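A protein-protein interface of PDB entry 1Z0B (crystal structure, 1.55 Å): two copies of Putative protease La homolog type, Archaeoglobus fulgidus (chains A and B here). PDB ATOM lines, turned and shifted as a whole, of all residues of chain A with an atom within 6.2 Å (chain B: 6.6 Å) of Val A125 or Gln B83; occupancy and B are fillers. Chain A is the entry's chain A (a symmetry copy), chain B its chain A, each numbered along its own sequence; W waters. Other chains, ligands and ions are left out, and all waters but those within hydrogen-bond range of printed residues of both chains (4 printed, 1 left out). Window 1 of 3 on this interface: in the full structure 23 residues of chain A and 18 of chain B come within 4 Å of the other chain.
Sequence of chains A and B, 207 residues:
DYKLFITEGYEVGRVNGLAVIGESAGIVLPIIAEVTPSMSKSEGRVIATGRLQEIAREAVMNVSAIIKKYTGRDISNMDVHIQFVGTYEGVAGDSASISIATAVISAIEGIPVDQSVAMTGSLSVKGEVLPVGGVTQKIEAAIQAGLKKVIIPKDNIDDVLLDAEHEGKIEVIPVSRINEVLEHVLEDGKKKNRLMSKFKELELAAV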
ATOM      1  N   MET A  61       9.179 -18.844   6.706  1.00  0.00           N
ATOM      2  CA  MET A  61       8.676 -19.859   7.644  1.00  0.00           C
ATOM      3  C   MET A  61       7.154 -19.992   7.540  1.00  0.00           C
ATOM      4  O   MET A  61       6.609 -21.104   7.485  1.00  0.00           O
ATOM      5  CB  MET A  61       9.116 -19.552   9.071  1.00  0.00           C
ATOM      6  CG  MET A  61      10.635 -19.731   9.236  1.00  0.00           C
ATOM      7  SD  MET A  61      11.145 -19.204  10.890  1.00  0.00           S
ATOM      8  CE  MET A  61      13.021 -19.209  10.521  1.00  0.00           C
ATOM      9  N   ASN A  62       6.452 -18.876   7.429  1.00  0.00           N
ATOM     10  CA  ASN A  62       4.987 -18.977   7.346  1.00  0.00           C
ATOM     11  C   ASN A  62       4.530 -19.638   6.063  1.00  0.00           C
ATOM     12  O   ASN A  62       3.632 -20.465   6.066  1.00  0.00           O
ATOM     13  CB  ASN A  62       4.330 -17.609   7.544  1.00  0.00           C
ATOM     14  CG  ASN A  62       4.578 -17.035   8.936  1.00  0.00           C
ATOM     15  OD1 ASN A  62       5.317 -17.603   9.760  1.00  0.00           O
ATOM     16  ND2 ASN A  62       3.979 -15.856   9.193  1.00  0.00           N
ATOM     17  N   VAL A  63       5.163 -19.303   4.940  1.00  0.00           N
ATOM     18  CA  VAL A  63       4.731 -19.902   3.679  1.00  0.00           C
ATOM     19  C   VAL A  63       5.116 -21.365   3.648  1.00  0.00           C
ATOM     20  O   VAL A  63       4.421 -22.153   3.033  1.00  0.00           O
ATOM     21  CB  VAL A  63       5.228 -19.095   2.455  1.00  0.00           C
ATOM     22  CG1 VAL A  63       6.663 -19.399   2.110  1.00  0.00           C
ATOM     23  CG2 VAL A  63       4.297 -19.291   1.274  1.00  0.00           C
ATOM     24  N   ALA A  65       4.836 -23.427   6.026  1.00  0.00           N
ATOM     25  CA  ALA A  65       3.741 -24.172   6.646  1.00  0.00           C
ATOM     26  C   ALA A  65       2.674 -24.519   5.645  1.00  0.00           C
ATOM     27  O   ALA A  65       2.253 -25.685   5.564  1.00  0.00           O
ATOM     28  CB  ALA A  65       3.158 -23.416   7.805  1.00  0.00           C
ATOM     29  N   ILE A  66       2.236 -23.542   4.845  1.00  0.00           N
ATOM     30  CA  ILE A  66       1.166 -23.806   3.877  1.00  0.00           C
ATOM     31  C   ILE A  66       1.651 -24.655   2.705  1.00  0.00           C
ATOM     32  O   ILE A  66       0.879 -25.439   2.141  1.00  0.00           O
ATOM     33  CB  ILE A  66       0.375 -22.528   3.417  1.00  0.00           C
ATOM     34  CG1 ILE A  66       1.181 -21.644   2.492  1.00  0.00           C
ATOM     35  CG2 ILE A  66      -0.172 -21.766   4.619  1.00  0.00           C
ATOM     36  CD1 ILE A  66       0.331 -20.506   1.944  1.00  0.00           C
ATOM     37  N   SER A  95       5.465  -7.378   8.096  1.00  0.00           N
ATOM     38  CA  SER A  95       5.740  -8.631   8.809  1.00  0.00           C
ATOM     39  C   SER A  95       5.267  -9.784   7.941  1.00  0.00           C
ATOM     40  O   SER A  95       4.198  -9.722   7.338  1.00  0.00           O
ATOM     41  CB  SER A  95       5.007  -8.664  10.142  1.00  0.00           C
ATOM     42  OG  SER A  95       5.346  -7.532  10.907  1.00  0.00           O
ATOM     43  N   ALA A  96       6.079 -10.822   7.852  1.00  0.00           N
ATOM     44  CA  ALA A  96       5.702 -11.988   7.066  1.00  0.00           C
ATOM     45  C   ALA A  96       5.191 -11.601   5.674  1.00  0.00           C
ATOM     46  O   ALA A  96       4.163 -12.109   5.202  1.00  0.00           O
ATOM     47  CB  ALA A  96       4.650 -12.805   7.808  1.00  0.00           C
ATOM     48  N   SER A 122       0.426  -9.243   5.205  1.00  0.00           N
ATOM     49  CA  SER A 122       1.234 -10.138   6.014  1.00  0.00           C
ATOM     50  C   SER A 122       0.593 -11.498   5.917  1.00  0.00           C
ATOM     51  O   SER A 122      -0.627 -11.611   6.022  1.00  0.00           O
ATOM     52  CB  SER A 122       1.216  -9.704   7.472  1.00  0.00           C
ATOM     53  OG  SER A 122       1.988  -8.518   7.663  1.00  0.00           O
ATOM     54  N   LEU A 123       1.402 -12.515   5.680  1.00  0.00           N
ATOM     55  CA  LEU A 123       0.877 -13.903   5.580  1.00  0.00           C
ATOM     56  C   LEU A 123       0.797 -14.569   6.953  1.00  0.00           C
ATOM     57  O   LEU A 123       1.810 -14.633   7.662  1.00  0.00           O
ATOM     58  CB  LEU A 123       1.770 -14.738   4.670  1.00  0.00           C
ATOM     59  CG  LEU A 123       1.183 -16.128   4.358  1.00  0.00           C
ATOM     60  CD1 LEU A 123      -0.100 -16.072   3.536  1.00  0.00           C
ATOM     61  CD2 LEU A 123       2.208 -17.039   3.728  1.00  0.00           C
ATOM     62  N   SER A 124      -0.392 -15.035   7.318  1.00  0.00           N
ATOM     63  CA  SER A 124      -0.508 -15.906   8.491  1.00  0.00           C
ATOM     64  C   SER A 124      -0.074 -17.324   8.157  1.00  0.00           C
ATOM     65  O   SER A 124      -0.152 -17.755   7.010  1.00  0.00           O
ATOM     66  CB  SER A 124      -1.916 -15.908   9.043  1.00  0.00           C
ATOM     67  OG  SER A 124      -2.714 -16.917   8.480  1.00  0.00           O
ATOM     68  N   VAL A 125       0.375 -18.058   9.168  1.00  0.00           N
ATOM     69  CA  VAL A 125       0.721 -19.477   8.989  1.00  0.00           C
ATOM     70  C   VAL A 125      -0.469 -20.328   8.529  1.00  0.00           C
ATOM     71  O   VAL A 125      -0.298 -21.460   8.098  1.00  0.00           O
ATOM     72  CB  VAL A 125       1.340 -20.080  10.271  1.00  0.00           C
ATOM     73  CG1 VAL A 125       2.713 -19.507  10.530  1.00  0.00           C
ATOM     74  CG2 VAL A 125       0.425 -19.875  11.494  1.00  0.00           C
ATOM     75  N   LYS A 126      -1.678 -19.784   8.620  1.00  0.00           N
ATOM     76  CA  LYS A 126      -2.898 -20.437   8.155  1.00  0.00           C
ATOM     77  C   LYS A 126      -3.273 -20.065   6.720  1.00  0.00           C
ATOM     78  O   LYS A 126      -4.250 -20.585   6.175  1.00  0.00           O
ATOM     79  CB  LYS A 126      -4.072 -20.134   9.095  1.00  0.00           C
ATOM     80  CG  LYS A 126      -3.885 -20.686  10.491  1.00  0.00           C
ATOM     81  CD  LYS A 126      -5.115 -21.428  10.988  1.00  0.00           C
ATOM     82  CE  LYS A 126      -5.649 -22.424   9.941  1.00  0.00           C
ATOM     83  NZ  LYS A 126      -5.737 -23.858  10.396  1.00  0.00           N
ATOM     84  N   GLY A 127      -2.516 -19.158   6.111  1.00  0.00           N
ATOM     85  CA  GLY A 127      -2.775 -18.753   4.726  1.00  0.00           C
ATOM     86  C   GLY A 127      -3.619 -17.489   4.583  1.00  0.00           C
ATOM     87  O   GLY A 127      -3.955 -17.095   3.463  1.00  0.00           O
ATOM     88  N   GLU A 128      -3.995 -16.870   5.701  1.00  0.00           N
ATOM     89  CA  GLU A 128      -4.750 -15.597   5.678  1.00  0.00           C
ATOM     90  C   GLU A 128      -3.821 -14.427   5.351  1.00  0.00           C
ATOM     91  O   GLU A 128      -2.615 -14.484   5.620  1.00  0.00           O
ATOM     92  CB  GLU A 128      -5.403 -15.302   7.040  1.00  0.00           C
ATOM     93  CG  GLU A 128      -6.152 -16.472   7.685  1.00  0.00           C
ATOM     94  CD  GLU A 128      -7.409 -16.899   6.936  1.00  0.00           C
ATOM     95  OE1 GLU A 128      -8.037 -16.071   6.232  1.00  0.00           O
ATOM     96  OE2 GLU A 128      -7.792 -18.081   7.058  1.00  0.00           O
ATOM     97  N   LEU A 130      -3.187 -10.751   6.459  1.00  0.00           N
ATOM     98  CA  LEU A 130      -3.448  -9.887   7.613  1.00  0.00           C
ATOM     99  C   LEU A 130      -3.107  -8.420   7.295  1.00  0.00           C
ATOM    100  O   LEU A 130      -2.200  -8.159   6.491  1.00  0.00           O
ATOM    101  CB  LEU A 130      -2.568 -10.363   8.762  1.00  0.00           C
ATOM    102  CG  LEU A 130      -3.024 -11.524   9.664  1.00  0.00           C
ATOM    103  CD1 LEU A 130      -4.110 -12.387   9.103  1.00  0.00           C
ATOM    104  CD2 LEU A 130      -1.794 -12.280  10.207  1.00  0.00           C
ATOM    105  N   GLY B  13      -6.668 -22.062  15.523  1.00  0.00           N
ATOM    106  CA  GLY B  13      -5.237 -21.804  15.650  1.00  0.00           C
ATOM    107  C   GLY B  13      -4.836 -20.392  16.010  1.00  0.00           C
ATOM    108  O   GLY B  13      -3.660 -20.082  15.983  1.00  0.00           O
ATOM    109  N   PRO B  30      -1.629 -11.403  19.601  1.00  0.00           N
ATOM    110  CA  PRO B  30      -2.215 -12.613  19.039  1.00  0.00           C
ATOM    111  C   PRO B  30      -1.158 -13.608  18.570  1.00  0.00           C
ATOM    112  O   PRO B  30      -0.086 -13.221  18.065  1.00  0.00           O
ATOM    113  CB  PRO B  30      -3.036 -12.102  17.842  1.00  0.00           C
ATOM    114  CG  PRO B  30      -3.179 -10.633  18.069  1.00  0.00           C
ATOM    115  CD  PRO B  30      -1.924 -10.214  18.776  1.00  0.00           C
ATOM    116  N   ILE B  31      -1.481 -14.882  18.743  1.00  0.00           N
ATOM    117  CA  ILE B  31      -0.648 -15.980  18.298  1.00  0.00           C
ATOM    118  C   ILE B  31      -1.432 -16.728  17.266  1.00  0.00           C
ATOM    119  O   ILE B  31      -2.616 -16.998  17.455  1.00  0.00           O
ATOM    120  CB  ILE B  31      -0.391 -17.002  19.443  1.00  0.00           C
ATOM    121  CG1 ILE B  31       0.093 -16.279  20.679  1.00  0.00           C
ATOM    122  CG2 ILE B  31       0.556 -18.141  18.976  1.00  0.00           C
ATOM    123  CD1 ILE B  31       1.491 -15.668  20.474  1.00  0.00           C
ATOM    124  N   ILE B  32      -0.775 -17.087  16.173  1.00  0.00           N
ATOM    125  CA  ILE B  32      -1.377 -18.013  15.217  1.00  0.00           C
ATOM    126  C   ILE B  32      -0.451 -19.223  15.105  1.00  0.00           C
ATOM    127  O   ILE B  32       0.793 -19.076  15.005  1.00  0.00           O
ATOM    128  CB  ILE B  32      -1.599 -17.389  13.833  1.00  0.00           C
ATOM    129  CG1 ILE B  32      -2.294 -16.033  13.970  1.00  0.00           C
ATOM    130  CG2 ILE B  32      -2.422 -18.324  12.994  1.00  0.00           C
ATOM    131  CD1 ILE B  32      -2.525 -15.302  12.654  1.00  0.00           C
ATOM    132  N   ALA B  33      -1.042 -20.423  15.188  1.00  0.00           N
ATOM    133  CA  ALA B  33      -0.259 -21.650  15.076  1.00  0.00           C
ATOM    134  C   ALA B  33      -0.774 -22.517  13.942  1.00  0.00           C
ATOM    135  O   ALA B  33      -1.962 -22.515  13.604  1.00  0.00           O
ATOM    136  CB  ALA B  33      -0.266 -22.428  16.377  1.00  0.00           C
ATOM    137  N   GLU B  34       0.148 -23.248  13.349  1.00  0.00           N
ATOM    138  CA  GLU B  34      -0.208 -24.261  12.355  1.00  0.00           C
ATOM    139  C   GLU B  34       0.676 -25.473  12.620  1.00  0.00           C
ATOM    140  O   GLU B  34       1.831 -25.328  13.046  1.00  0.00           O
ATOM    141  CB  GLU B  34       0.000 -23.747  10.915  1.00  0.00           C
ATOM    142  CG  GLU B  34      -0.465 -24.714   9.824  1.00  0.00           C
ATOM    143  CD  GLU B  34      -1.914 -25.164  10.014  1.00  0.00           C
ATOM    144  OE1 GLU B  34      -2.192 -25.995  10.908  1.00  0.00           O
ATOM    145  OE2 GLU B  34      -2.806 -24.686   9.293  1.00  0.00           O
ATOM    146  N   ILE B  47       8.957 -24.272  14.624  1.00  0.00           N
ATOM    147  CA  ILE B  47       9.381 -23.267  13.685  1.00  0.00           C
ATOM    148  C   ILE B  47       8.859 -21.893  14.112  1.00  0.00           C
ATOM    149  O   ILE B  47       7.651 -21.603  14.040  1.00  0.00           O
ATOM    150  CB  ILE B  47       8.962 -23.639  12.274  1.00  0.00           C
ATOM    151  CG1 ILE B  47       9.641 -24.969  11.875  1.00  0.00           C
ATOM    152  CG2 ILE B  47       9.348 -22.545  11.311  1.00  0.00           C
ATOM    153  CD1 ILE B  47       9.068 -25.639  10.656  1.00  0.00           C
ATOM    154  N   ALA B  48       9.781 -21.056  14.574  1.00  0.00           N
ATOM    155  CA  ALA B  48       9.435 -19.733  15.084  1.00  0.00           C
ATOM    156  C   ALA B  48      10.641 -18.826  14.891  1.00  0.00           C
ATOM    157  O   ALA B  48      11.775 -19.285  14.837  1.00  0.00           O
ATOM    158  CB  ALA B  48       9.061 -19.816  16.556  1.00  0.00           C
ATOM    159  N   HIS B  81       4.386 -24.513  13.733  1.00  0.00           N
ATOM    160  CA  HIS B  81       4.729 -23.140  13.341  1.00  0.00           C
ATOM    161  C   HIS B  81       4.025 -22.186  14.266  1.00  0.00           C
ATOM    162  O   HIS B  81       2.782 -22.234  14.376  1.00  0.00           O
ATOM    163  CB  HIS B  81       4.268 -22.845  11.909  1.00  0.00           C
ATOM    164  CG  HIS B  81       5.032 -23.591  10.854  1.00  0.00           C
ATOM    165  ND1 HIS B  81       5.925 -22.972  10.003  1.00  0.00           N
ATOM    166  CD2 HIS B  81       5.028 -24.900  10.508  1.00  0.00           C
ATOM    167  CE1 HIS B  81       6.458 -23.872   9.194  1.00  0.00           C
ATOM    168  NE2 HIS B  81       5.927 -25.053   9.476  1.00  0.00           N
ATOM    169  N   ILE B  82       4.809 -21.308  14.900  1.00  0.00           N
ATOM    170  CA  ILE B  82       4.260 -20.275  15.797  1.00  0.00           C
ATOM    171  C   ILE B  82       4.538 -18.878  15.223  1.00  0.00           C
ATOM    172  O   ILE B  82       5.697 -18.524  14.931  1.00  0.00           O
ATOM    173  CB  ILE B  82       4.846 -20.380  17.225  1.00  0.00           C
ATOM    174  CG1 ILE B  82       4.639 -21.798  17.795  1.00  0.00           C
ATOM    175  CG2 ILE B  82       4.255 -19.314  18.128  1.00  0.00           C
ATOM    176  CD1 ILE B  82       3.175 -22.189  17.888  1.00  0.00           C
ATOM    177  N   GLN B  83       3.468 -18.109  15.067  1.00  0.00           N
ATOM    178  CA  GLN B  83       3.534 -16.737  14.582  1.00  0.00           C
ATOM    179  C   GLN B  83       3.010 -15.781  15.623  1.00  0.00           C
ATOM    180  O   GLN B  83       1.917 -15.954  16.141  1.00  0.00           O
ATOM    181  CB  GLN B  83       2.680 -16.612  13.332  1.00  0.00           C
ATOM    182  CG  GLN B  83       2.398 -15.158  12.872  1.00  0.00           C
ATOM    183  CD  GLN B  83       1.713 -15.118  11.559  1.00  0.00           C
ATOM    184  OE1 GLN B  83       1.014 -16.044  11.183  1.00  0.00           O
ATOM    185  NE2 GLN B  83       1.910 -14.029  10.819  1.00  0.00           N
ATOM    186  N   PHE B  84       3.796 -14.753  15.921  1.00  0.00           N
ATOM    187  CA  PHE B  84       3.371 -13.669  16.779  1.00  0.00           C
ATOM    188  C   PHE B  84       2.902 -12.537  15.879  1.00  0.00           C
ATOM    189  O   PHE B  84       3.653 -12.086  15.005  1.00  0.00           O
ATOM    190  CB  PHE B  84       4.533 -13.218  17.641  1.00  0.00           C
ATOM    191  CG  PHE B  84       5.030 -14.287  18.595  1.00  0.00           C
ATOM    192  CD1 PHE B  84       4.419 -14.474  19.832  1.00  0.00           C
ATOM    193  CD2 PHE B  84       6.091 -15.119  18.253  1.00  0.00           C
ATOM    194  CE1 PHE B  84       4.865 -15.479  20.734  1.00  0.00           C
ATOM    195  CE2 PHE B  84       6.568 -16.119  19.148  1.00  0.00           C
ATOM    196  CZ  PHE B  84       5.951 -16.292  20.388  1.00  0.00           C
ATOM    197  N   VAL B  85       1.662 -12.111  16.051  1.00  0.00           N
ATOM    198  CA  VAL B  85       1.098 -11.033  15.234  1.00  0.00           C
ATOM    199  C   VAL B  85       1.400  -9.648  15.832  1.00  0.00           C
ATOM    200  O   VAL B  85       0.952  -9.308  16.933  1.00  0.00           O
ATOM    201  CB  VAL B  85      -0.401 -11.216  15.052  1.00  0.00           C
ATOM    202  CG1 VAL B  85      -0.943 -10.137  14.168  1.00  0.00           C
ATOM    203  CG2 VAL B  85      -0.692 -12.569  14.445  1.00  0.00           C
HETATM  204  O   HOH W   1      -4.715 -23.589   6.954  1.00  0.00           O
HETATM  205  O   HOH W   2      -4.670 -26.274  11.653  1.00  0.00           O
HETATM  206  O   HOH W   3      -3.993 -23.768  12.308  1.00  0.00           O
HETATM  207  O   HOH W   4      -2.219 -23.590   6.976  1.00  0.00           O
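CG of Met A61 touches CG2 of Ile B47, 3.7 Å away. Met A61 touches Ala B48. Ser A124 touches Ile B32 (CB to CD1, 3.7 Å). Ser A124 touches Gln B83 (CA to OE1, 3.1 Å). Val A125 touches Ile B32 (CG2 to CG2, 3.6 Å). CG2 of Val A125 touches C of Ala B33 (3.8 Å). Val A125 touches Glu B34. His B81 touches Val A125 (CB to CG1, 3.9 Å). Lys A126 touches Ile B32. CD2 of Leu A130 touches CD1 of Ile B32, at 3.96 Å.
Water W3 lies within hydrogen-bond range of NZ of Lys A126, O of Ala B33 and OE1 of Glu B34. Water W2 lies within hydrogen-bond range of the side-chain carboxylate (OE1) of Glu B34 (2.6 Å) and the side-chain amino group (NZ) of Lys A126 (2.9 Å). Water W4 bridges OE2 of Glu B34 (2.6 Å) and O of Val A125 (3.1 Å). Water W1 bridges the backbone carbonyl oxygen (O) of Lys A126 (3.1 Å) and the side-chain carboxylate (OE2) of Glu B34 (3.2 Å).
Of the 15 printed residues of chain A, 8 touch a printed residue of chain B. Hydrophobic or aromatic side chains of chain A that line the printed part of chain B: Met A61, Ala A65, Val A125 and Leu A130. Hydrophobic or aromatic side chains of chain B within 4 Å of the printed part of chain A: Ile B32, Ile B47 and His B81. Among the printed residues, 16 pairs touch across the chains. Among the printed residues, Asp or Glu carboxylates within 4 Å of a Lys or Arg side-chain nitrogen of the other chain: Lys A126 with Glu B34.
No position is printed for both chains. Of the 16 pairs that touch across the chains among the printed residues, none has its exchanged pair printed and touching as well.
NZ of Lys A126 lies within salt-bridge range of OE2 of Glu B34 (3.2 Å). ND1 of His B81 sits at hydrogen-bond distance from O of Met A61 (3.2 Å). NE2 of Gln B83 sits close to ND2 of Asn A62 (3.2 Å). The backbone carbonyl oxygen of Leu A123 sits at hydrogen-bond distance from the side-chain amide nitrogen of Gln B83, 3.2 Å away. The side-chain amide oxygen of Gln B83 lies within hydrogen-bond range of the backbone NH of Val A125 (2.9 Å).
The backbone NH of Ala B33 lies within hydrogen-bond range of the backbone carbonyl oxygen of Gly B13, at 2.8 Å. O of Ile B32 sits at hydrogen-bond distance from N of Gln B83, 2.8 Å away. N of His B81 lies within hydrogen-bond range of O of Glu B34 (2.8 Å). The backbone carbonyl oxygen (O) of Leu A123 is in hydrogen-bond range of the side-chain amide nitrogen (ND2) of Asn A62 (2.9 Å). N of Lys A126 sits close to OG of Ser A124 (3.1 Å). The side-chain hydroxyl (OG) of Ser A124 sits at hydrogen-bond distance from the backbone NH (N) of Glu A128 (3.1 Å).
Printed residues of chain B within 4 Å of Asn A62: Gln B83. Ala A96 touches none of the printed residues of chain B. Val A125 touches five residues of chain B. Gly A127 touches none of the printed residues of chain B. Of the printed residues of chain B, Leu A130 touches Ile B32 (3.96 Å). Gln B83 touches just these residues of chain A: Asn A62, Leu A123, Ser A124 and Val A125. The nearest residue of chain B that does not touch Val A125 is Ile B82 (5.1 Å).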
